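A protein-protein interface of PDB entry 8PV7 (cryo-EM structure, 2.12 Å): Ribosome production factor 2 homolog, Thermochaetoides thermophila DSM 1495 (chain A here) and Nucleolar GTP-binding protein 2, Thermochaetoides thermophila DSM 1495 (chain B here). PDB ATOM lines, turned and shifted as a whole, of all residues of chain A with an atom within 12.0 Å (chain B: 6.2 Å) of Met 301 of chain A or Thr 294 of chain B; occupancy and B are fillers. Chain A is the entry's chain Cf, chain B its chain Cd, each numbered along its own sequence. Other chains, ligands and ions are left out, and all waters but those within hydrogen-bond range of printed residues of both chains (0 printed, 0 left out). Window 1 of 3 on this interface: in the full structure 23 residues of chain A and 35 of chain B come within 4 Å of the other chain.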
ATOM      1  N   ASN A 286      -9.767   0.911 -21.703  1.00  0.00           N
ATOM      2  CA  ASN A 286      -9.566   0.241 -20.418  1.00  0.00           C
ATOM      3  C   ASN A 286     -10.866  -0.188 -19.748  1.00  0.00           C
ATOM      4  O   ASN A 286     -10.861  -0.504 -18.556  1.00  0.00           O
ATOM      5  CB  ASN A 286      -8.745   1.104 -19.449  1.00  0.00           C
ATOM      6  CG  ASN A 286      -7.333   1.332 -19.929  1.00  0.00           C
ATOM      7  OD1 ASN A 286      -6.700   0.428 -20.462  1.00  0.00           O
ATOM      8  ND2 ASN A 286      -6.839   2.550 -19.761  1.00  0.00           N
ATOM      9  N   GLY A 297     -12.609  -2.499 -15.167  1.00  0.00           N
ATOM     10  CA  GLY A 297     -11.653  -1.476 -15.538  1.00  0.00           C
ATOM     11  C   GLY A 297     -10.233  -1.995 -15.437  1.00  0.00           C
ATOM     12  O   GLY A 297      -9.929  -2.848 -14.605  1.00  0.00           O
ATOM     13  N   ARG A 298      -9.363  -1.468 -16.292  1.00  0.00           N
ATOM     14  CA  ARG A 298      -7.960  -1.853 -16.343  1.00  0.00           C
ATOM     15  C   ARG A 298      -7.100  -0.721 -15.806  1.00  0.00           C
ATOM     16  O   ARG A 298      -7.243   0.429 -16.233  1.00  0.00           O
ATOM     17  CB  ARG A 298      -7.537  -2.190 -17.771  1.00  0.00           C
ATOM     18  CG  ARG A 298      -7.540  -3.660 -18.078  1.00  0.00           C
ATOM     19  CD  ARG A 298      -6.290  -4.328 -17.553  1.00  0.00           C
ATOM     20  NE  ARG A 298      -6.301  -5.756 -17.848  1.00  0.00           N
ATOM     21  CZ  ARG A 298      -5.417  -6.623 -17.377  1.00  0.00           C
ATOM     22  NH1 ARG A 298      -4.418  -6.239 -16.603  1.00  0.00           N
ATOM     23  NH2 ARG A 298      -5.544  -7.909 -17.689  1.00  0.00           N
ATOM     24  N   ILE A 299      -6.214  -1.044 -14.876  1.00  0.00           N
ATOM     25  CA  ILE A 299      -5.223  -0.097 -14.389  1.00  0.00           C
ATOM     26  C   ILE A 299      -3.851  -0.577 -14.829  1.00  0.00           C
ATOM     27  O   ILE A 299      -3.617  -1.777 -15.007  1.00  0.00           O
ATOM     28  CB  ILE A 299      -5.276   0.085 -12.858  1.00  0.00           C
ATOM     29  CG1 ILE A 299      -5.169  -1.266 -12.155  1.00  0.00           C
ATOM     30  CG2 ILE A 299      -6.545   0.811 -12.459  1.00  0.00           C
ATOM     31  CD1 ILE A 299      -5.060  -1.160 -10.665  1.00  0.00           C
ATOM     32  N   HIS A 300      -2.940   0.370 -15.012  1.00  0.00           N
ATOM     33  CA  HIS A 300      -1.593   0.088 -15.495  1.00  0.00           C
ATOM     34  C   HIS A 300      -0.593   0.672 -14.511  1.00  0.00           C
ATOM     35  O   HIS A 300      -0.474   1.894 -14.388  1.00  0.00           O
ATOM     36  CB  HIS A 300      -1.405   0.639 -16.903  1.00  0.00           C
ATOM     37  CG  HIS A 300      -2.481   0.210 -17.845  1.00  0.00           C
ATOM     38  ND1 HIS A 300      -2.508  -1.043 -18.418  1.00  0.00           N
ATOM     39  CD2 HIS A 300      -3.593   0.847 -18.281  1.00  0.00           C
ATOM     40  CE1 HIS A 300      -3.578  -1.150 -19.181  1.00  0.00           C
ATOM     41  NE2 HIS A 300      -4.254  -0.019 -19.115  1.00  0.00           N
ATOM     42  N   MET A 301       0.113  -0.213 -13.808  1.00  0.00           N
ATOM     43  CA  MET A 301       0.961   0.205 -12.700  1.00  0.00           C
ATOM     44  C   MET A 301       2.245   0.850 -13.199  1.00  0.00           C
ATOM     45  O   MET A 301       2.723   1.834 -12.624  1.00  0.00           O
ATOM     46  CB  MET A 301       1.276  -1.001 -11.820  1.00  0.00           C
ATOM     47  CG  MET A 301       0.176  -1.341 -10.844  1.00  0.00           C
ATOM     48  SD  MET A 301      -0.468   0.115 -10.029  1.00  0.00           S
ATOM     49  CE  MET A 301       0.779   0.310  -8.774  1.00  0.00           C
ATOM     50  N   GLY A 302       2.820   0.306 -14.261  1.00  0.00           N
ATOM     51  CA  GLY A 302       4.123   0.729 -14.721  1.00  0.00           C
ATOM     52  C   GLY A 302       5.238  -0.086 -14.087  1.00  0.00           C
ATOM     53  O   GLY A 302       5.047  -0.811 -13.108  1.00  0.00           O
ATOM     54  N   LYS A 303       6.427   0.032 -14.668  1.00  0.00           N
ATOM     55  CA  LYS A 303       7.579  -0.693 -14.155  1.00  0.00           C
ATOM     56  C   LYS A 303       8.087  -0.049 -12.873  1.00  0.00           C
ATOM     57  O   LYS A 303       8.236   1.173 -12.787  1.00  0.00           O
ATOM     58  CB  LYS A 303       8.691  -0.733 -15.203  1.00  0.00           C
ATOM     59  N   THR A 304       8.345  -0.881 -11.867  1.00  0.00           N
ATOM     60  CA  THR A 304       8.878  -0.402 -10.598  1.00  0.00           C
ATOM     61  C   THR A 304      10.388  -0.238 -10.718  1.00  0.00           C
ATOM     62  O   THR A 304      11.113  -1.225 -10.878  1.00  0.00           O
ATOM     63  CB  THR A 304       8.528  -1.371  -9.471  1.00  0.00           C
ATOM     64  N   ASP A 305      10.861   1.005 -10.641  1.00  0.00           N
ATOM     65  CA  ASP A 305      12.275   1.328 -10.823  1.00  0.00           C
ATOM     66  C   ASP A 305      12.785   2.010  -9.557  1.00  0.00           C
ATOM     67  O   ASP A 305      12.631   3.223  -9.392  1.00  0.00           O
ATOM     68  CB  ASP A 305      12.485   2.211 -12.049  1.00  0.00           C
ATOM     69  N   LEU A 306      13.407   1.230  -8.681  1.00  0.00           N
ATOM     70  CA  LEU A 306      13.945   1.723  -7.422  1.00  0.00           C
ATOM     71  C   LEU A 306      15.427   2.056  -7.504  1.00  0.00           C
ATOM     72  O   LEU A 306      16.066   2.239  -6.464  1.00  0.00           O
ATOM     73  CB  LEU A 306      13.704   0.697  -6.312  1.00  0.00           C
ATOM     74  CG  LEU A 306      12.472   0.844  -5.416  1.00  0.00           C
ATOM     75  CD1 LEU A 306      11.202   1.098  -6.207  1.00  0.00           C
ATOM     76  CD2 LEU A 306      12.313  -0.401  -4.571  1.00  0.00           C
ATOM     77  N   TYR B 103      -4.734  -6.439 -11.489  1.00  0.00           N
ATOM     78  CA  TYR B 103      -4.720  -5.222 -12.286  1.00  0.00           C
ATOM     79  C   TYR B 103      -6.068  -4.907 -12.911  1.00  0.00           C
ATOM     80  O   TYR B 103      -6.148  -4.029 -13.775  1.00  0.00           O
ATOM     81  CB  TYR B 103      -3.645  -5.318 -13.364  1.00  0.00           C
ATOM     82  CG  TYR B 103      -2.312  -5.747 -12.814  1.00  0.00           C
ATOM     83  CD1 TYR B 103      -1.737  -5.075 -11.744  1.00  0.00           C
ATOM     84  CD2 TYR B 103      -1.639  -6.835 -13.345  1.00  0.00           C
ATOM     85  CE1 TYR B 103      -0.521  -5.464 -11.231  1.00  0.00           C
ATOM     86  CE2 TYR B 103      -0.423  -7.233 -12.837  1.00  0.00           C
ATOM     87  CZ  TYR B 103       0.132  -6.546 -11.780  1.00  0.00           C
ATOM     88  OH  TYR B 103       1.346  -6.941 -11.271  1.00  0.00           O
ATOM     89  N   VAL B 267      -5.560  -0.520  -2.818  1.00  0.00           N
ATOM     90  CA  VAL B 267      -4.196  -0.367  -3.308  1.00  0.00           C
ATOM     91  C   VAL B 267      -3.244  -0.316  -2.120  1.00  0.00           C
ATOM     92  O   VAL B 267      -3.441   0.478  -1.196  1.00  0.00           O
ATOM     93  CB  VAL B 267      -4.051   0.903  -4.174  1.00  0.00           C
ATOM     94  CG1 VAL B 267      -2.592   1.175  -4.505  1.00  0.00           C
ATOM     95  CG2 VAL B 267      -4.875   0.785  -5.445  1.00  0.00           C
ATOM     96  N   PHE B 268      -2.213  -1.161  -2.145  1.00  0.00           N
ATOM     97  CA  PHE B 268      -1.154  -1.131  -1.144  1.00  0.00           C
ATOM     98  C   PHE B 268      -0.179  -0.004  -1.445  1.00  0.00           C
ATOM     99  O   PHE B 268       0.213   0.204  -2.594  1.00  0.00           O
ATOM    100  CB  PHE B 268      -0.382  -2.451  -1.113  1.00  0.00           C
ATOM    101  CG  PHE B 268      -1.049  -3.533  -0.333  1.00  0.00           C
ATOM    102  CD1 PHE B 268      -1.544  -3.291   0.932  1.00  0.00           C
ATOM    103  CD2 PHE B 268      -1.157  -4.807  -0.858  1.00  0.00           C
ATOM    104  CE1 PHE B 268      -2.155  -4.294   1.651  1.00  0.00           C
ATOM    105  CE2 PHE B 268      -1.764  -5.814  -0.142  1.00  0.00           C
ATOM    106  CZ  PHE B 268      -2.265  -5.556   1.114  1.00  0.00           C
ATOM    107  N   VAL B 269       0.238   0.704  -0.403  1.00  0.00           N
ATOM    108  CA  VAL B 269       1.307   1.688  -0.507  1.00  0.00           C
ATOM    109  C   VAL B 269       2.368   1.313   0.518  1.00  0.00           C
ATOM    110  O   VAL B 269       2.153   1.464   1.724  1.00  0.00           O
ATOM    111  CB  VAL B 269       0.818   3.126  -0.285  1.00  0.00           C
ATOM    112  CG1 VAL B 269       1.967   4.089  -0.456  1.00  0.00           C
ATOM    113  CG2 VAL B 269      -0.296   3.469  -1.250  1.00  0.00           C
ATOM    114  N   LEU B 270       3.502   0.818   0.040  1.00  0.00           N
ATOM    115  CA  LEU B 270       4.643   0.519   0.893  1.00  0.00           C
ATOM    116  C   LEU B 270       5.409   1.812   1.144  1.00  0.00           C
ATOM    117  O   LEU B 270       6.118   2.299   0.258  1.00  0.00           O
ATOM    118  CB  LEU B 270       5.525  -0.534   0.230  1.00  0.00           C
ATOM    119  CG  LEU B 270       6.442  -1.392   1.095  1.00  0.00           C
ATOM    120  CD1 LEU B 270       5.656  -2.168   2.130  1.00  0.00           C
ATOM    121  CD2 LEU B 270       7.245  -2.332   0.221  1.00  0.00           C
ATOM    122  N   TRP B 284       9.440  -7.337  -1.486  1.00  0.00           N
ATOM    123  CA  TRP B 284       8.160  -7.185  -0.804  1.00  0.00           C
ATOM    124  C   TRP B 284       7.080  -6.676  -1.751  1.00  0.00           C
ATOM    125  O   TRP B 284       5.914  -7.064  -1.629  1.00  0.00           O
ATOM    126  CB  TRP B 284       8.306  -6.256   0.399  1.00  0.00           C
ATOM    127  CG  TRP B 284       8.794  -6.934   1.637  1.00  0.00           C
ATOM    128  CD1 TRP B 284       9.980  -6.724   2.269  1.00  0.00           C
ATOM    129  CD2 TRP B 284       8.105  -7.930   2.398  1.00  0.00           C
ATOM    130  NE1 TRP B 284      10.077  -7.529   3.373  1.00  0.00           N
ATOM    131  CE2 TRP B 284       8.936  -8.276   3.478  1.00  0.00           C
ATOM    132  CE3 TRP B 284       6.864  -8.558   2.276  1.00  0.00           C
ATOM    133  CZ2 TRP B 284       8.570  -9.226   4.423  1.00  0.00           C
ATOM    134  CZ3 TRP B 284       6.504  -9.498   3.212  1.00  0.00           C
ATOM    135  CH2 TRP B 284       7.352  -9.825   4.272  1.00  0.00           C
ATOM    136  N   ILE B 285       7.448  -5.815  -2.705  1.00  0.00           N
ATOM    137  CA  ILE B 285       6.492  -5.375  -3.720  1.00  0.00           C
ATOM    138  C   ILE B 285       6.039  -6.551  -4.574  1.00  0.00           C
ATOM    139  O   ILE B 285       4.847  -6.687  -4.880  1.00  0.00           O
ATOM    140  CB  ILE B 285       7.099  -4.248  -4.576  1.00  0.00           C
ATOM    141  CG1 ILE B 285       7.104  -2.942  -3.798  1.00  0.00           C
ATOM    142  CG2 ILE B 285       6.322  -4.044  -5.858  1.00  0.00           C
ATOM    143  CD1 ILE B 285       7.836  -1.856  -4.507  1.00  0.00           C
ATOM    144  N   LEU B 288       3.542  -8.522  -2.496  1.00  0.00           N
ATOM    145  CA  LEU B 288       2.246  -7.881  -2.273  1.00  0.00           C
ATOM    146  C   LEU B 288       1.436  -7.737  -3.558  1.00  0.00           C
ATOM    147  O   LEU B 288       0.197  -7.714  -3.512  1.00  0.00           O
ATOM    148  CB  LEU B 288       2.449  -6.516  -1.621  1.00  0.00           C
ATOM    149  CG  LEU B 288       3.008  -6.551  -0.200  1.00  0.00           C
ATOM    150  CD1 LEU B 288       3.506  -5.182   0.206  1.00  0.00           C
ATOM    151  CD2 LEU B 288       1.976  -7.062   0.785  1.00  0.00           C
ATOM    152  N   GLN B 289       2.105  -7.640  -4.707  1.00  0.00           N
ATOM    153  CA  GLN B 289       1.388  -7.463  -5.962  1.00  0.00           C
ATOM    154  C   GLN B 289       0.689  -8.732  -6.430  1.00  0.00           C
ATOM    155  O   GLN B 289      -0.073  -8.673  -7.398  1.00  0.00           O
ATOM    156  CB  GLN B 289       2.338  -6.951  -7.043  1.00  0.00           C
ATOM    157  CG  GLN B 289       3.312  -7.984  -7.560  1.00  0.00           C
ATOM    158  CD  GLN B 289       4.384  -7.375  -8.435  1.00  0.00           C
ATOM    159  OE1 GLN B 289       4.470  -6.157  -8.572  1.00  0.00           O
ATOM    160  NE2 GLN B 289       5.209  -8.224  -9.034  1.00  0.00           N
ATOM    161  N   LYS B 290       0.935  -9.870  -5.784  1.00  0.00           N
ATOM    162  CA  LYS B 290       0.139 -11.058  -6.061  1.00  0.00           C
ATOM    163  C   LYS B 290      -1.297 -10.882  -5.592  1.00  0.00           C
ATOM    164  O   LYS B 290      -2.216 -11.459  -6.181  1.00  0.00           O
ATOM    165  CB  LYS B 290       0.771 -12.280  -5.400  1.00  0.00           C
ATOM    166  CG  LYS B 290       2.179 -12.569  -5.881  1.00  0.00           C
ATOM    167  CD  LYS B 290       2.217 -13.744  -6.831  1.00  0.00           C
ATOM    168  CE  LYS B 290       3.639 -14.039  -7.282  1.00  0.00           C
ATOM    169  NZ  LYS B 290       4.648 -13.521  -6.321  1.00  0.00           N
ATOM    170  N   HIS B 292      -2.670  -7.376  -4.379  1.00  0.00           N
ATOM    171  CA  HIS B 292      -3.213  -6.067  -4.715  1.00  0.00           C
ATOM    172  C   HIS B 292      -2.124  -5.192  -5.317  1.00  0.00           C
ATOM    173  O   HIS B 292      -0.941  -5.400  -5.028  1.00  0.00           O
ATOM    174  CB  HIS B 292      -3.815  -5.389  -3.473  1.00  0.00           C
ATOM    175  CG  HIS B 292      -5.056  -6.057  -2.971  1.00  0.00           C
ATOM    176  ND1 HIS B 292      -5.046  -6.959  -1.931  1.00  0.00           N
ATOM    177  CD2 HIS B 292      -6.343  -5.965  -3.378  1.00  0.00           C
ATOM    178  CE1 HIS B 292      -6.275  -7.389  -1.714  1.00  0.00           C
ATOM    179  NE2 HIS B 292      -7.081  -6.804  -2.581  1.00  0.00           N
ATOM    180  N   PRO B 293      -2.486  -4.228  -6.168  1.00  0.00           N
ATOM    181  CA  PRO B 293      -1.475  -3.331  -6.749  1.00  0.00           C
ATOM    182  C   PRO B 293      -0.752  -2.528  -5.678  1.00  0.00           C
ATOM    183  O   PRO B 293      -1.369  -2.005  -4.752  1.00  0.00           O
ATOM    184  CB  PRO B 293      -2.299  -2.420  -7.661  1.00  0.00           C
ATOM    185  CG  PRO B 293      -3.543  -3.147  -7.917  1.00  0.00           C
ATOM    186  CD  PRO B 293      -3.828  -3.949  -6.706  1.00  0.00           C
ATOM    187  N   THR B 294       0.566  -2.414  -5.823  1.00  0.00           N
ATOM    188  CA  THR B 294       1.423  -1.873  -4.778  1.00  0.00           C
ATOM    189  C   THR B 294       2.281  -0.742  -5.321  1.00  0.00           C
ATOM    190  O   THR B 294       2.882  -0.865  -6.390  1.00  0.00           O
ATOM    191  CB  THR B 294       2.316  -2.972  -4.186  1.00  0.00           C
ATOM    192  OG1 THR B 294       1.507  -4.095  -3.825  1.00  0.00           O
ATOM    193  CG2 THR B 294       3.049  -2.472  -2.955  1.00  0.00           C
ATOM    194  N   CYS B 295       2.331   0.359  -4.578  1.00  0.00           N
ATOM    195  CA  CYS B 295       3.167   1.506  -4.905  1.00  0.00           C
ATOM    196  C   CYS B 295       4.226   1.687  -3.830  1.00  0.00           C
ATOM    197  O   CYS B 295       3.910   1.705  -2.640  1.00  0.00           O
ATOM    198  CB  CYS B 295       2.345   2.794  -5.009  1.00  0.00           C
ATOM    199  SG  CYS B 295       0.987   2.774  -6.179  1.00  0.00           S
ATOM    200  N   ALA B 296       5.477   1.844  -4.242  1.00  0.00           N
ATOM    201  CA  ALA B 296       6.553   2.199  -3.327  1.00  0.00           C
ATOM    202  C   ALA B 296       6.584   3.707  -3.138  1.00  0.00           C
ATOM    203  O   ALA B 296       6.472   4.464  -4.106  1.00  0.00           O
ATOM    204  CB  ALA B 296       7.904   1.716  -3.843  1.00  0.00           C
ATOM    205  N   SER B 309       4.153   8.233  -9.765  1.00  0.00           N
ATOM    206  CA  SER B 309       3.497   6.953 -10.015  1.00  0.00           C
ATOM    207  C   SER B 309       2.163   6.856  -9.281  1.00  0.00           C
ATOM    208  O   SER B 309       1.156   6.409  -9.851  1.00  0.00           O
ATOM    209  CB  SER B 309       4.431   5.815  -9.607  1.00  0.00           C
ATOM    210  OG  SER B 309       3.755   4.572  -9.598  1.00  0.00           O
ATOM    211  N   LEU B 313      -1.619   6.636 -10.969  1.00  0.00           N
ATOM    212  CA  LEU B 313      -2.604   5.602 -10.648  1.00  0.00           C
ATOM    213  C   LEU B 313      -3.941   6.212 -10.231  1.00  0.00           C
ATOM    214  O   LEU B 313      -5.012   5.757 -10.664  1.00  0.00           O
ATOM    215  CB  LEU B 313      -2.067   4.685  -9.551  1.00  0.00           C
ATOM    216  CG  LEU B 313      -2.989   3.535  -9.148  1.00  0.00           C
ATOM    217  CD1 LEU B 313      -3.358   2.685 -10.352  1.00  0.00           C
ATOM    218  CD2 LEU B 313      -2.364   2.685  -8.061  1.00  0.00           C
ATOM    219  N   GLN B 316      -5.725   7.458 -13.270  1.00  0.00           N
ATOM    220  CA  GLN B 316      -6.381   6.361 -13.976  1.00  0.00           C
ATOM    221  C   GLN B 316      -7.709   5.997 -13.325  1.00  0.00           C
ATOM    222  O   GLN B 316      -8.700   5.751 -14.023  1.00  0.00           O
ATOM    223  CB  GLN B 316      -5.469   5.139 -14.030  1.00  0.00           C
ATOM    224  CG  GLN B 316      -4.223   5.326 -14.852  1.00  0.00           C
ATOM    225  CD  GLN B 316      -3.373   4.081 -14.897  1.00  0.00           C
ATOM    226  OE1 GLN B 316      -3.882   2.973 -15.005  1.00  0.00           O
ATOM    227  NE2 GLN B 316      -2.068   4.255 -14.780  1.00  0.00           N
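The side-chain amide oxygen (OE1) of Gln 316 of chain B sits at hydrogen-bond distance from the backbone NH (N) of His 300 of chain A.
N of Ile 299 of chain A sits at hydrogen-bond distance from O of Tyr 103 of chain B, 3.2 Å away.
The backbone NH of Arg 298 of chain A lies within hydrogen-bond range of the backbone carbonyl oxygen of Asn 286 of chain A, 2.9 Å away.
The backbone carbonyl oxygen (O) of His 292 of chain B is in hydrogen-bond range of the side-chain hydroxyl (OG1) of Thr 294 of chain B (3.0 Å).
O of Pro 293 of chain B is in hydrogen-bond range of N of Phe 268 of chain B (2.9 Å).
OD1 of Asn 286 of chain A is in hydrogen-bond range of NE2 of His 300 of chain A (2.8 Å).
The backbone carbonyl oxygen (O) of Phe 268 of chain B is in hydrogen-bond range of the backbone NH (N) of Cys 295 of chain B (2.9 Å).
The backbone NH (N) of Leu 270 of chain B sits at hydrogen-bond distance from the backbone carbonyl oxygen (O) of Cys 295 of chain B (2.9 Å).
Among the printed residues, pairs that only touch across the chains: Met 301 of chain A with Thr 294 of chain B, Ile 299 of chain A with Gln 316 of chain B, Arg 298 of chain A with Tyr 103 of chain B, Met 301 of chain A with Cys 295 of chain B, Ile 299 of chain A with Pro 293 of chain B, Met 301 of chain A with Leu 313 of chain B and Met 301 of chain A with Pro 293 of chain B.
Of the printed residues of chain B, Arg 298 of chain A touches Tyr 103.
Of the printed residues of chain B, Ile 299 of chain A touches Tyr 103, Pro 293 and Gln 316.
Printed residues of chain B within 4 Å of His 300 of chain A: Gln 316.
Of chain B, only Pro 293 (3.9 Å), Thr 294 (3.4 Å), Cys 295 (3.6 Å) and Leu 313 (3.8 Å) come within 4 Å of Met 301 of chain A.
Of the printed residues of chain A, Tyr 103 of chain B touches Arg 298 and Ile 299.
No residue of chain A comes within 4 Å of Val 267 of chain B.
No residue of chain A comes within 4 Å of Val 269 of chain B.
No residue of chain A comes within 4 Å of Leu 270 of chain B.
No residue of chain A comes within 4 Å of Leu 288 of chain B.
Of chain A, only Ile 299 and Met 301 come within 4 Å of Pro 293 of chain B.
Thr 294 of chain B touches one residue of chain A.
Cys 295 of chain B touches one residue of chain A.
Ala 296 of chain B touches none of the printed residues of chain A.
No residue of chain A comes within 4 Å of Ser 309 of chain B.
Printed residues of chain A within 4 Å of Gln 316 of chain B: Ile 299 and His 300.
The nearest printed residue of chain B that does not touch Arg 298 of chain A is Gln 316 of chain B (4.4 Å).
Of the 11 printed residues of chain A, 4 touch a printed residue of chain B.
Printed residues of chain A that touch a printed residue of chain B: Arg 298, Ile 299, His 300 and Met 301.
Hydrophobic or aromatic side chains of chain A within 4 Å of the printed part of chain B: Ile 299, His 300 and Met 301.
Among the printed residues, 9 pairs touch across the chains.
Among the printed residues, no Asp or Glu carboxylate lies within 4 Å of a Lys or Arg side-chain nitrogen of the other chain.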
